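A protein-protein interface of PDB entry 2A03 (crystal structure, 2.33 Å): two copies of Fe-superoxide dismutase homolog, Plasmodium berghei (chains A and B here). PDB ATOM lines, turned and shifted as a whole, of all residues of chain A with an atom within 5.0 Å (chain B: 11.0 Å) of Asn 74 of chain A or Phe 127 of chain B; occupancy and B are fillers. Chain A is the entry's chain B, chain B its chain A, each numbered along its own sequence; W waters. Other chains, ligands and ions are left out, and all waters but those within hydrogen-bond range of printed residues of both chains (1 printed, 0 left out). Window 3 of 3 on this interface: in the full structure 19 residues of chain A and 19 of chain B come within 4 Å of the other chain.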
ATOM      1  N   TYR A  43      22.363  -8.030  18.779  1.00  0.00           N
ATOM      2  CA  TYR A  43      20.956  -8.420  18.753  1.00  0.00           C
ATOM      3  C   TYR A  43      20.322  -8.108  17.383  1.00  0.00           C
ATOM      4  O   TYR A  43      19.570  -8.910  16.828  1.00  0.00           O
ATOM      5  CB  TYR A  43      20.181  -7.703  19.862  1.00  0.00           C
ATOM      6  CG  TYR A  43      20.521  -8.109  21.286  1.00  0.00           C
ATOM      7  CD1 TYR A  43      20.414  -9.436  21.707  1.00  0.00           C
ATOM      8  CD2 TYR A  43      20.901  -7.149  22.231  1.00  0.00           C
ATOM      9  CE1 TYR A  43      20.696  -9.798  23.046  1.00  0.00           C
ATOM     10  CE2 TYR A  43      21.199  -7.497  23.566  1.00  0.00           C
ATOM     11  CZ  TYR A  43      21.096  -8.813  23.961  1.00  0.00           C
ATOM     12  OH  TYR A  43      21.378  -9.149  25.269  1.00  0.00           O
ATOM     13  N   GLY A  70      10.640 -17.638  20.823  1.00  0.00           N
ATOM     14  CA  GLY A  70      11.999 -18.164  20.943  1.00  0.00           C
ATOM     15  C   GLY A  70      13.098 -17.124  20.800  1.00  0.00           C
ATOM     16  O   GLY A  70      12.951 -15.987  21.241  1.00  0.00           O
ATOM     17  N   ALA A  71      14.198 -17.525  20.169  1.00  0.00           N
ATOM     18  CA  ALA A  71      15.355 -16.655  20.010  1.00  0.00           C
ATOM     19  C   ALA A  71      15.057 -15.491  19.077  1.00  0.00           C
ATOM     20  O   ALA A  71      15.647 -14.416  19.217  1.00  0.00           O
ATOM     21  CB  ALA A  71      16.587 -17.459  19.523  1.00  0.00           C
ATOM     22  N   ILE A  72      14.143 -15.684  18.126  1.00  0.00           N
ATOM     23  CA  ILE A  72      13.755 -14.573  17.268  1.00  0.00           C
ATOM     24  C   ILE A  72      13.119 -13.480  18.133  1.00  0.00           C
ATOM     25  O   ILE A  72      13.515 -12.313  18.053  1.00  0.00           O
ATOM     26  CB  ILE A  72      12.836 -15.017  16.119  1.00  0.00           C
ATOM     27  CG1 ILE A  72      13.653 -15.820  15.094  1.00  0.00           C
ATOM     28  CG2 ILE A  72      12.194 -13.820  15.432  1.00  0.00           C
ATOM     29  CD1 ILE A  72      12.858 -16.347  13.937  1.00  0.00           C
ATOM     30  N   PHE A  73      12.169 -13.861  18.986  1.00  0.00           N
ATOM     31  CA  PHE A  73      11.562 -12.902  19.901  1.00  0.00           C
ATOM     32  C   PHE A  73      12.590 -12.261  20.827  1.00  0.00           C
ATOM     33  O   PHE A  73      12.619 -11.034  20.981  1.00  0.00           O
ATOM     34  CB  PHE A  73      10.468 -13.520  20.772  1.00  0.00           C
ATOM     35  CG  PHE A  73       9.929 -12.552  21.773  1.00  0.00           C
ATOM     36  CD1 PHE A  73       9.024 -11.580  21.386  1.00  0.00           C
ATOM     37  CD2 PHE A  73      10.400 -12.542  23.071  1.00  0.00           C
ATOM     38  CE1 PHE A  73       8.558 -10.638  22.288  1.00  0.00           C
ATOM     39  CE2 PHE A  73       9.935 -11.593  23.990  1.00  0.00           C
ATOM     40  CZ  PHE A  73       9.029 -10.639  23.587  1.00  0.00           C
ATOM     41  N   ASN A  74      13.425 -13.105  21.442  1.00  0.00           N
ATOM     42  CA  ASN A  74      14.423 -12.646  22.377  1.00  0.00           C
ATOM     43  C   ASN A  74      15.349 -11.555  21.798  1.00  0.00           C
ATOM     44  O   ASN A  74      15.624 -10.558  22.462  1.00  0.00           O
ATOM     45  CB  ASN A  74      15.240 -13.830  22.905  1.00  0.00           C
ATOM     46  CG  ASN A  74      14.465 -14.675  23.922  1.00  0.00           C
ATOM     47  OD1 ASN A  74      13.456 -14.241  24.443  1.00  0.00           O
ATOM     48  ND2 ASN A  74      14.950 -15.877  24.200  1.00  0.00           N
ATOM     49  N   ASN A  75      15.839 -11.755  20.580  1.00  0.00           N
ATOM     50  CA  ASN A  75      16.704 -10.772  19.938  1.00  0.00           C
ATOM     51  C   ASN A  75      15.961  -9.507  19.550  1.00  0.00           C
ATOM     52  O   ASN A  75      16.424  -8.399  19.843  1.00  0.00           O
ATOM     53  CB  ASN A  75      17.389 -11.374  18.718  1.00  0.00           C
ATOM     54  CG  ASN A  75      18.570 -12.263  19.092  1.00  0.00           C
ATOM     55  OD1 ASN A  75      19.653 -11.764  19.397  1.00  0.00           O
ATOM     56  ND2 ASN A  75      18.370 -13.587  19.044  1.00  0.00           N
ATOM     57  N   ALA A  76      14.814  -9.667  18.895  1.00  0.00           N
ATOM     58  CA  ALA A  76      13.944  -8.529  18.588  1.00  0.00           C
ATOM     59  C   ALA A  76      13.583  -7.668  19.825  1.00  0.00           C
ATOM     60  O   ALA A  76      13.659  -6.444  19.788  1.00  0.00           O
ATOM     61  CB  ALA A  76      12.676  -9.017  17.908  1.00  0.00           C
ATOM     62  N   ALA A  77      13.164  -8.314  20.903  1.00  0.00           N
ATOM     63  CA  ALA A  77      12.800  -7.611  22.120  1.00  0.00           C
ATOM     64  C   ALA A  77      14.025  -6.929  22.765  1.00  0.00           C
ATOM     65  O   ALA A  77      13.928  -5.785  23.227  1.00  0.00           O
ATOM     66  CB  ALA A  77      12.141  -8.554  23.085  1.00  0.00           C
ATOM     67  N   GLN A  78      15.180  -7.589  22.757  1.00  0.00           N
ATOM     68  CA  GLN A  78      16.387  -6.929  23.259  1.00  0.00           C
ATOM     69  C   GLN A  78      16.753  -5.666  22.463  1.00  0.00           C
ATOM     70  O   GLN A  78      17.222  -4.678  23.045  1.00  0.00           O
ATOM     71  CB  GLN A  78      17.579  -7.894  23.337  1.00  0.00           C
ATOM     72  CG  GLN A  78      17.485  -8.899  24.481  1.00  0.00           C
ATOM     73  CD  GLN A  78      17.587  -8.253  25.856  1.00  0.00           C
ATOM     74  OE1 GLN A  78      16.611  -7.689  26.369  1.00  0.00           O
ATOM     75  NE2 GLN A  78      18.789  -8.326  26.460  1.00  0.00           N
ATOM     76  N   ASP A 149      15.209 -11.458  31.648  1.00  0.00           N
ATOM     77  CA  ASP A 149      15.850 -11.635  30.350  1.00  0.00           C
ATOM     78  C   ASP A 149      15.391 -10.580  29.320  1.00  0.00           C
ATOM     79  O   ASP A 149      15.700  -9.402  29.482  1.00  0.00           O
ATOM     80  CB  ASP A 149      15.633 -13.078  29.860  1.00  0.00           C
ATOM     81  CG  ASP A 149      16.236 -14.127  30.809  1.00  0.00           C
ATOM     82  OD1 ASP A 149      17.128 -13.806  31.611  1.00  0.00           O
ATOM     83  OD2 ASP A 149      15.824 -15.299  30.743  1.00  0.00           O
ATOM     84  N   ALA A 150      14.659 -10.982  28.280  1.00  0.00           N
ATOM     85  CA  ALA A 150      14.208 -10.056  27.221  1.00  0.00           C
ATOM     86  C   ALA A 150      12.784  -9.538  27.419  1.00  0.00           C
ATOM     87  O   ALA A 150      12.260  -8.812  26.571  1.00  0.00           O
ATOM     88  CB  ALA A 150      14.308 -10.720  25.865  1.00  0.00           C
ATOM     89  N   TRP A 168      20.938  -6.423  33.410  1.00  0.00           N
ATOM     90  CA  TRP A 168      21.862  -7.469  32.975  1.00  0.00           C
ATOM     91  C   TRP A 168      23.267  -7.055  33.458  1.00  0.00           C
ATOM     92  O   TRP A 168      23.627  -5.853  33.442  1.00  0.00           O
ATOM     93  CB  TRP A 168      21.859  -7.606  31.465  1.00  0.00           C
ATOM     94  CG  TRP A 168      20.668  -8.316  30.836  1.00  0.00           C
ATOM     95  CD1 TRP A 168      19.338  -7.945  30.897  1.00  0.00           C
ATOM     96  CD2 TRP A 168      20.724  -9.450  29.961  1.00  0.00           C
ATOM     97  NE1 TRP A 168      18.565  -8.825  30.151  1.00  0.00           N
ATOM     98  CE2 TRP A 168      19.392  -9.748  29.564  1.00  0.00           C
ATOM     99  CE3 TRP A 168      21.772 -10.257  29.487  1.00  0.00           C
ATOM    100  CZ2 TRP A 168      19.087 -10.814  28.716  1.00  0.00           C
ATOM    101  CZ3 TRP A 168      21.468 -11.320  28.651  1.00  0.00           C
ATOM    102  CH2 TRP A 168      20.129 -11.591  28.281  1.00  0.00           C
ATOM    103  N   SER B 120      29.464 -27.061  23.923  1.00  0.00           N
ATOM    104  CA  SER B 120      29.849 -25.705  23.559  1.00  0.00           C
ATOM    105  C   SER B 120      28.684 -24.968  22.939  1.00  0.00           C
ATOM    106  O   SER B 120      28.462 -23.789  23.229  1.00  0.00           O
ATOM    107  CB  SER B 120      31.008 -25.742  22.551  1.00  0.00           C
ATOM    108  OG  SER B 120      32.181 -26.290  23.143  1.00  0.00           O
ATOM    109  N   ASN B 121      27.962 -25.644  22.045  1.00  0.00           N
ATOM    110  CA  ASN B 121      26.786 -25.050  21.399  1.00  0.00           C
ATOM    111  C   ASN B 121      25.717 -24.663  22.434  1.00  0.00           C
ATOM    112  O   ASN B 121      25.178 -23.554  22.404  1.00  0.00           O
ATOM    113  CB  ASN B 121      26.207 -25.997  20.342  1.00  0.00           C
ATOM    114  CG  ASN B 121      27.094 -26.113  19.099  1.00  0.00           C
ATOM    115  OD1 ASN B 121      27.809 -25.185  18.743  1.00  0.00           O
ATOM    116  ND2 ASN B 121      27.056 -27.263  18.451  1.00  0.00           N
ATOM    117  N   VAL B 122      25.459 -25.563  23.373  1.00  0.00           N
ATOM    118  CA  VAL B 122      24.508 -25.311  24.455  1.00  0.00           C
ATOM    119  C   VAL B 122      24.959 -24.162  25.383  1.00  0.00           C
ATOM    120  O   VAL B 122      24.154 -23.301  25.762  1.00  0.00           O
ATOM    121  CB  VAL B 122      24.282 -26.613  25.286  1.00  0.00           C
ATOM    122  CG1 VAL B 122      23.611 -26.316  26.631  1.00  0.00           C
ATOM    123  CG2 VAL B 122      23.460 -27.621  24.477  1.00  0.00           C
ATOM    124  N   LEU B 123      26.232 -24.167  25.763  1.00  0.00           N
ATOM    125  CA  LEU B 123      26.807 -23.105  26.595  1.00  0.00           C
ATOM    126  C   LEU B 123      26.739 -21.724  25.925  1.00  0.00           C
ATOM    127  O   LEU B 123      26.464 -20.708  26.585  1.00  0.00           O
ATOM    128  CB  LEU B 123      28.267 -23.420  26.914  1.00  0.00           C
ATOM    129  CG  LEU B 123      28.501 -24.585  27.874  1.00  0.00           C
ATOM    130  CD1 LEU B 123      29.993 -24.901  27.985  1.00  0.00           C
ATOM    131  CD2 LEU B 123      27.873 -24.314  29.236  1.00  0.00           C
ATOM    132  N   CYS B 124      27.001 -21.699  24.623  1.00  0.00           N
ATOM    133  CA  CYS B 124      26.987 -20.451  23.842  1.00  0.00           C
ATOM    134  C   CYS B 124      25.618 -19.945  23.442  1.00  0.00           C
ATOM    135  O   CYS B 124      25.444 -18.766  23.268  1.00  0.00           O
ATOM    136  CB  CYS B 124      27.823 -20.602  22.575  1.00  0.00           C
ATOM    137  SG  CYS B 124      29.575 -20.661  22.925  1.00  0.00           S
ATOM    138  N   GLY B 125      24.656 -20.831  23.267  1.00  0.00           N
ATOM    139  CA  GLY B 125      23.311 -20.416  22.883  1.00  0.00           C
ATOM    140  C   GLY B 125      22.397 -20.093  24.065  1.00  0.00           C
ATOM    141  O   GLY B 125      21.292 -19.609  23.871  1.00  0.00           O
ATOM    142  N   HIS B 126      22.828 -20.360  25.291  1.00  0.00           N
ATOM    143  CA  HIS B 126      21.954 -20.101  26.427  1.00  0.00           C
ATOM    144  C   HIS B 126      21.695 -18.598  26.617  1.00  0.00           C
ATOM    145  O   HIS B 126      22.621 -17.792  26.753  1.00  0.00           O
ATOM    146  CB  HIS B 126      22.521 -20.698  27.716  1.00  0.00           C
ATOM    147  CG  HIS B 126      21.598 -20.547  28.884  1.00  0.00           C
ATOM    148  ND1 HIS B 126      20.627 -21.478  29.186  1.00  0.00           N
ATOM    149  CD2 HIS B 126      21.452 -19.546  29.781  1.00  0.00           C
ATOM    150  CE1 HIS B 126      19.932 -21.061  30.228  1.00  0.00           C
ATOM    151  NE2 HIS B 126      20.410 -19.889  30.607  1.00  0.00           N
ATOM    152  N   PHE B 127      20.428 -18.226  26.633  1.00  0.00           N
ATOM    153  CA  PHE B 127      20.048 -16.828  26.705  1.00  0.00           C
ATOM    154  C   PHE B 127      19.807 -16.435  28.153  1.00  0.00           C
ATOM    155  O   PHE B 127      19.079 -17.118  28.872  1.00  0.00           O
ATOM    156  CB  PHE B 127      18.803 -16.570  25.859  1.00  0.00           C
ATOM    157  CG  PHE B 127      18.417 -15.129  25.786  1.00  0.00           C
ATOM    158  CD1 PHE B 127      19.196 -14.228  25.078  1.00  0.00           C
ATOM    159  CD2 PHE B 127      17.285 -14.666  26.441  1.00  0.00           C
ATOM    160  CE1 PHE B 127      18.844 -12.880  25.012  1.00  0.00           C
ATOM    161  CE2 PHE B 127      16.928 -13.320  26.373  1.00  0.00           C
ATOM    162  CZ  PHE B 127      17.707 -12.427  25.659  1.00  0.00           C
ATOM    163  N   GLY B 128      20.436 -15.333  28.570  1.00  0.00           N
ATOM    164  CA  GLY B 128      20.374 -14.879  29.938  1.00  0.00           C
ATOM    165  C   GLY B 128      21.339 -15.615  30.860  1.00  0.00           C
ATOM    166  O   GLY B 128      22.327 -16.206  30.424  1.00  0.00           O
ATOM    167  N   SER B 129      21.046 -15.563  32.151  1.00  0.00           N
ATOM    168  CA  SER B 129      21.873 -16.192  33.170  1.00  0.00           C
ATOM    169  C   SER B 129      21.545 -17.667  33.276  1.00  0.00           C
ATOM    170  O   SER B 129      20.396 -18.073  33.148  1.00  0.00           O
ATOM    171  CB  SER B 129      21.640 -15.502  34.514  1.00  0.00           C
ATOM    172  OG  SER B 129      21.890 -14.106  34.399  1.00  0.00           O
ATOM    173  N   GLY B 130      22.568 -18.487  33.484  1.00  0.00           N
ATOM    174  CA  GLY B 130      22.346 -19.912  33.605  1.00  0.00           C
ATOM    175  C   GLY B 130      23.604 -20.746  33.727  1.00  0.00           C
ATOM    176  O   GLY B 130      24.695 -20.243  34.044  1.00  0.00           O
ATOM    177  N   TRP B 131      23.402 -22.044  33.492  1.00  0.00           N
ATOM    178  CA  TRP B 131      24.392 -23.070  33.667  1.00  0.00           C
ATOM    179  C   TRP B 131      24.213 -24.136  32.586  1.00  0.00           C
ATOM    180  O   TRP B 131      23.092 -24.439  32.158  1.00  0.00           O
ATOM    181  CB  TRP B 131      24.182 -23.740  35.029  1.00  0.00           C
ATOM    182  CG  TRP B 131      24.265 -22.808  36.197  1.00  0.00           C
ATOM    183  CD1 TRP B 131      23.260 -22.061  36.716  1.00  0.00           C
ATOM    184  CD2 TRP B 131      25.418 -22.541  36.990  1.00  0.00           C
ATOM    185  NE1 TRP B 131      23.719 -21.315  37.768  1.00  0.00           N
ATOM    186  CE2 TRP B 131      25.042 -21.593  37.962  1.00  0.00           C
ATOM    187  CE3 TRP B 131      26.744 -22.999  36.965  1.00  0.00           C
ATOM    188  CZ2 TRP B 131      25.940 -21.099  38.914  1.00  0.00           C
ATOM    189  CZ3 TRP B 131      27.635 -22.498  37.899  1.00  0.00           C
ATOM    190  CH2 TRP B 131      27.228 -21.563  38.864  1.00  0.00           C
ATOM    191  N   GLY B 132      25.331 -24.706  32.147  1.00  0.00           N
ATOM    192  CA  GLY B 132      25.323 -25.941  31.369  1.00  0.00           C
ATOM    193  C   GLY B 132      25.815 -27.082  32.243  1.00  0.00           C
ATOM    194  O   GLY B 132      26.654 -26.884  33.114  1.00  0.00           O
ATOM    195  N   GLN B 146      20.752 -27.774  30.414  1.00  0.00           N
ATOM    196  CA  GLN B 146      20.962 -26.382  30.756  1.00  0.00           C
ATOM    197  C   GLN B 146      19.853 -25.919  31.683  1.00  0.00           C
ATOM    198  O   GLN B 146      18.730 -26.412  31.622  1.00  0.00           O
ATOM    199  CB  GLN B 146      21.029 -25.504  29.505  1.00  0.00           C
ATOM    200  CG  GLN B 146      19.733 -25.446  28.689  1.00  0.00           C
ATOM    201  CD  GLN B 146      19.884 -24.630  27.408  1.00  0.00           C
ATOM    202  OE1 GLN B 146      20.292 -23.469  27.431  1.00  0.00           O
ATOM    203  NE2 GLN B 146      19.539 -25.231  26.295  1.00  0.00           N
ATOM    204  N   THR B 147      20.198 -24.981  32.557  1.00  0.00           N
ATOM    205  CA  THR B 147      19.261 -24.422  33.508  1.00  0.00           C
ATOM    206  C   THR B 147      19.394 -22.907  33.526  1.00  0.00           C
ATOM    207  O   THR B 147      20.397 -22.347  33.126  1.00  0.00           O
ATOM    208  CB  THR B 147      19.495 -24.961  34.936  1.00  0.00           C
ATOM    209  OG1 THR B 147      20.812 -24.602  35.386  1.00  0.00           O
ATOM    210  CG2 THR B 147      19.293 -26.479  34.992  1.00  0.00           C
ATOM    211  N   HIS B 148      18.332 -22.263  33.974  1.00  0.00           N
ATOM    212  CA  HIS B 148      18.243 -20.826  34.009  1.00  0.00           C
ATOM    213  C   HIS B 148      18.506 -20.366  35.428  1.00  0.00           C
ATOM    214  O   HIS B 148      18.039 -20.988  36.388  1.00  0.00           O
ATOM    215  CB  HIS B 148      16.868 -20.381  33.547  1.00  0.00           C
ATOM    216  CG  HIS B 148      16.859 -19.014  32.951  1.00  0.00           C
ATOM    217  ND1 HIS B 148      17.721 -18.644  31.937  1.00  0.00           N
ATOM    218  CD2 HIS B 148      16.115 -17.921  33.238  1.00  0.00           C
ATOM    219  CE1 HIS B 148      17.495 -17.385  31.614  1.00  0.00           C
ATOM    220  NE2 HIS B 148      16.526 -16.923  32.387  1.00  0.00           N
ATOM    221  N   ASP B 149      19.211 -19.244  35.534  1.00  0.00           N
ATOM    222  CA  ASP B 149      19.467 -18.591  36.798  1.00  0.00           C
ATOM    223  C   ASP B 149      20.135 -19.516  37.828  1.00  0.00           C
ATOM    224  O   ASP B 149      21.324 -19.827  37.680  1.00  0.00           O
ATOM    225  CB  ASP B 149      18.171 -17.942  37.287  1.00  0.00           C
ATOM    226  CG  ASP B 149      17.733 -16.791  36.386  1.00  0.00           C
ATOM    227  OD1 ASP B 149      18.574 -16.223  35.656  1.00  0.00           O
ATOM    228  OD2 ASP B 149      16.550 -16.431  36.414  1.00  0.00           O
ATOM    229  N   ALA B 150      19.393 -19.964  38.845  1.00  0.00           N
ATOM    230  CA  ALA B 150      19.953 -20.789  39.934  1.00  0.00           C
ATOM    231  C   ALA B 150      19.646 -22.250  39.763  1.00  0.00           C
ATOM    232  O   ALA B 150      20.034 -23.072  40.605  1.00  0.00           O
ATOM    233  CB  ALA B 150      19.445 -20.329  41.287  1.00  0.00           C
ATOM    234  N   ASP B 166      29.492 -22.318  34.461  1.00  0.00           N
ATOM    235  CA  ASP B 166      28.708 -21.106  34.700  1.00  0.00           C
ATOM    236  C   ASP B 166      28.703 -20.230  33.434  1.00  0.00           C
ATOM    237  O   ASP B 166      29.759 -19.879  32.921  1.00  0.00           O
ATOM    238  CB  ASP B 166      29.371 -20.355  35.866  1.00  0.00           C
ATOM    239  CG  ASP B 166      28.498 -19.251  36.464  1.00  0.00           C
ATOM    240  OD1 ASP B 166      27.391 -18.967  35.955  1.00  0.00           O
ATOM    241  OD2 ASP B 166      28.933 -18.667  37.486  1.00  0.00           O
ATOM    242  N   VAL B 167      27.519 -19.853  32.952  1.00  0.00           N
ATOM    243  CA  VAL B 167      27.426 -18.853  31.894  1.00  0.00           C
ATOM    244  C   VAL B 167      26.680 -17.566  32.292  1.00  0.00           C
ATOM    245  O   VAL B 167      26.325 -16.788  31.431  1.00  0.00           O
ATOM    246  CB  VAL B 167      26.856 -19.431  30.565  1.00  0.00           C
ATOM    247  CG1 VAL B 167      27.738 -20.600  30.053  1.00  0.00           C
ATOM    248  CG2 VAL B 167      25.413 -19.864  30.704  1.00  0.00           C
ATOM    249  N   TRP B 168      26.482 -17.310  33.586  1.00  0.00           N
ATOM    250  CA  TRP B 168      26.183 -15.918  34.020  1.00  0.00           C
ATOM    251  C   TRP B 168      27.289 -15.007  33.477  1.00  0.00           C
ATOM    252  O   TRP B 168      28.472 -15.387  33.488  1.00  0.00           O
ATOM    253  CB  TRP B 168      26.156 -15.779  35.544  1.00  0.00           C
ATOM    254  CG  TRP B 168      24.942 -16.373  36.208  1.00  0.00           C
ATOM    255  CD1 TRP B 168      24.498 -17.675  36.127  1.00  0.00           C
ATOM    256  CD2 TRP B 168      24.019 -15.695  37.066  1.00  0.00           C
ATOM    257  NE1 TRP B 168      23.360 -17.830  36.876  1.00  0.00           N
ATOM    258  CE2 TRP B 168      23.046 -16.636  37.462  1.00  0.00           C
ATOM    259  CE3 TRP B 168      23.917 -14.384  37.533  1.00  0.00           C
ATOM    260  CZ2 TRP B 168      21.990 -16.301  38.305  1.00  0.00           C
ATOM    261  CZ3 TRP B 168      22.881 -14.063  38.367  1.00  0.00           C
ATOM    262  CH2 TRP B 168      21.928 -15.014  38.745  1.00  0.00           C
ATOM    263  N   GLU B 169      26.928 -13.802  33.041  1.00  0.00           N
ATOM    264  CA  GLU B 169      27.914 -12.883  32.461  1.00  0.00           C
ATOM    265  C   GLU B 169      29.120 -12.628  33.394  1.00  0.00           C
ATOM    266  O   GLU B 169      30.242 -12.421  32.907  1.00  0.00           O
ATOM    267  CB  GLU B 169      27.258 -11.573  32.006  1.00  0.00           C
ATOM    268  CG  GLU B 169      26.482 -11.761  30.725  1.00  0.00           C
ATOM    269  CD  GLU B 169      25.644 -10.564  30.270  1.00  0.00           C
ATOM    270  OE1 GLU B 169      25.103  -9.801  31.111  1.00  0.00           O
ATOM    271  OE2 GLU B 169      25.483 -10.424  29.037  1.00  0.00           O
ATOM    272  N   TYR B 172      32.532 -14.432  33.101  1.00  0.00           N
ATOM    273  CA  TYR B 172      33.469 -14.155  32.002  1.00  0.00           C
ATOM    274  C   TYR B 172      33.633 -12.697  31.576  1.00  0.00           C
ATOM    275  O   TYR B 172      34.532 -12.384  30.813  1.00  0.00           O
ATOM    276  CB  TYR B 172      33.098 -15.014  30.781  1.00  0.00           C
ATOM    277  CG  TYR B 172      31.725 -14.748  30.181  1.00  0.00           C
ATOM    278  CD1 TYR B 172      31.526 -13.728  29.234  1.00  0.00           C
ATOM    279  CD2 TYR B 172      30.626 -15.536  30.538  1.00  0.00           C
ATOM    280  CE1 TYR B 172      30.265 -13.505  28.685  1.00  0.00           C
ATOM    281  CE2 TYR B 172      29.381 -15.322  30.000  1.00  0.00           C
ATOM    282  CZ  TYR B 172      29.196 -14.317  29.063  1.00  0.00           C
ATOM    283  OH  TYR B 172      27.939 -14.124  28.534  1.00  0.00           O
ATOM    284  N   ARG B 180      31.453 -14.686  24.870  1.00  0.00           N
ATOM    285  CA  ARG B 180      31.272 -15.957  25.577  1.00  0.00           C
ATOM    286  C   ARG B 180      31.979 -17.141  24.882  1.00  0.00           C
ATOM    287  O   ARG B 180      32.433 -18.087  25.540  1.00  0.00           O
ATOM    288  CB  ARG B 180      29.784 -16.271  25.743  1.00  0.00           C
ATOM    289  CG  ARG B 180      29.522 -17.254  26.864  1.00  0.00           C
ATOM    290  CD  ARG B 180      28.100 -17.775  26.818  1.00  0.00           C
ATOM    291  NE  ARG B 180      27.142 -16.769  27.262  1.00  0.00           N
ATOM    292  CZ  ARG B 180      25.830 -16.970  27.347  1.00  0.00           C
ATOM    293  NH1 ARG B 180      25.301 -18.151  27.017  1.00  0.00           N
ATOM    294  NH2 ARG B 180      25.043 -15.984  27.756  1.00  0.00           N
HETATM  295  O   HOH W   1      18.621 -14.572  33.636  1.00  0.00           O
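A ring nitrogen (NE2) of His 148 of chain B is in hydrogen-bond range of the side-chain carboxylate (OD2) of Asp 149 of chain A (2.4 Å).
NE2 of His 126 of chain B sits at hydrogen-bond distance from ND1 of His 148 of chain B (3.2 Å). The backbone carbonyl oxygen (O) of Ser 129 of chain B lies within hydrogen-bond range of a ring nitrogen (ND1) of His 148 of chain B (3.0 Å). NE2 of Gln 78 of chain A is in hydrogen-bond range of OH of Tyr 43 of chain A. The backbone carbonyl oxygen (O) of Asp 149 of chain A sits at hydrogen-bond distance from the indole nitrogen (NE1) of Trp 168 of chain A (3.0 Å).
CD2 of Phe 127 of chain B touches ND2 of Asn 74 of chain A (3.5 Å). Gln 78 of chain A touches Phe 127 of chain B (CG to CZ, 3.7 Å). Phe 127 of chain B touches Asp 149 of chain A. OD1 of Asp 149 of chain A touches CA of Gly 128 of chain B (3.8 Å). CB of Ala 150 of chain A touches CE2 of Phe 127 of chain B (3.7 Å). Phe 127 of chain B touches Trp 168 of chain A. Trp 168 of chain A touches Gly 128 of chain B. Trp 168 of chain A touches Glu 169 of chain B.
No residue of chain B comes within 4 Å of Ala 71 of chain A. No residue of chain B comes within 4 Å of Phe 73 of chain A. Of chain B, only Phe 127 comes within 4 Å of Asn 74 of chain A. No residue of chain B comes within 4 Å of Asn 75 of chain A. No residue of chain B comes within 4 Å of Ala 77 of chain A. Of chain B, only Phe 127 (3.7 Å) comes within 4 Å of Gln 78 of chain A. Of the printed residues of chain B, Trp 168 of chain A touches Phe 127 (3.7 Å), Gly 128 (3.7 Å) and Glu 169 (3.7 Å). Printed residues of chain A within 4 Å of Gly 128 of chain B: Asp 149 and Trp 168. Printed residues of chain A within 4 Å of His 148 of chain B: Asp 149 (2.4 Å). Printed residues of chain A within 4 Å of Glu 169 of chain B: Trp 168. The nearest residue of chain B that does not touch Asn 74 of chain A is Gly 128 of chain B (7.0 Å). The nearest residue of chain A that does not touch Phe 127 of chain B is Tyr 43 of chain A (4.1 Å).
Of the 24 printed residues of chain B, 4 touch a printed residue of chain A. Among the printed residues, no Asp or Glu carboxylate lies within 4 Å of a Lys or Arg side-chain nitrogen of the other chain.
3 positions are printed for both chains.
Water W1 lies within hydrogen-bond range of the side-chain carboxylate (OD1) of Asp 149 of chain B (2.6 Å), the side-chain carboxylate (OD1) of Asp 149 of chain A (2.6 Å), the backbone NH (N) of Ser 129 of chain B (3.0 Å) and a ring nitrogen (NE2) of His 148 of chain B (3.4 Å).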
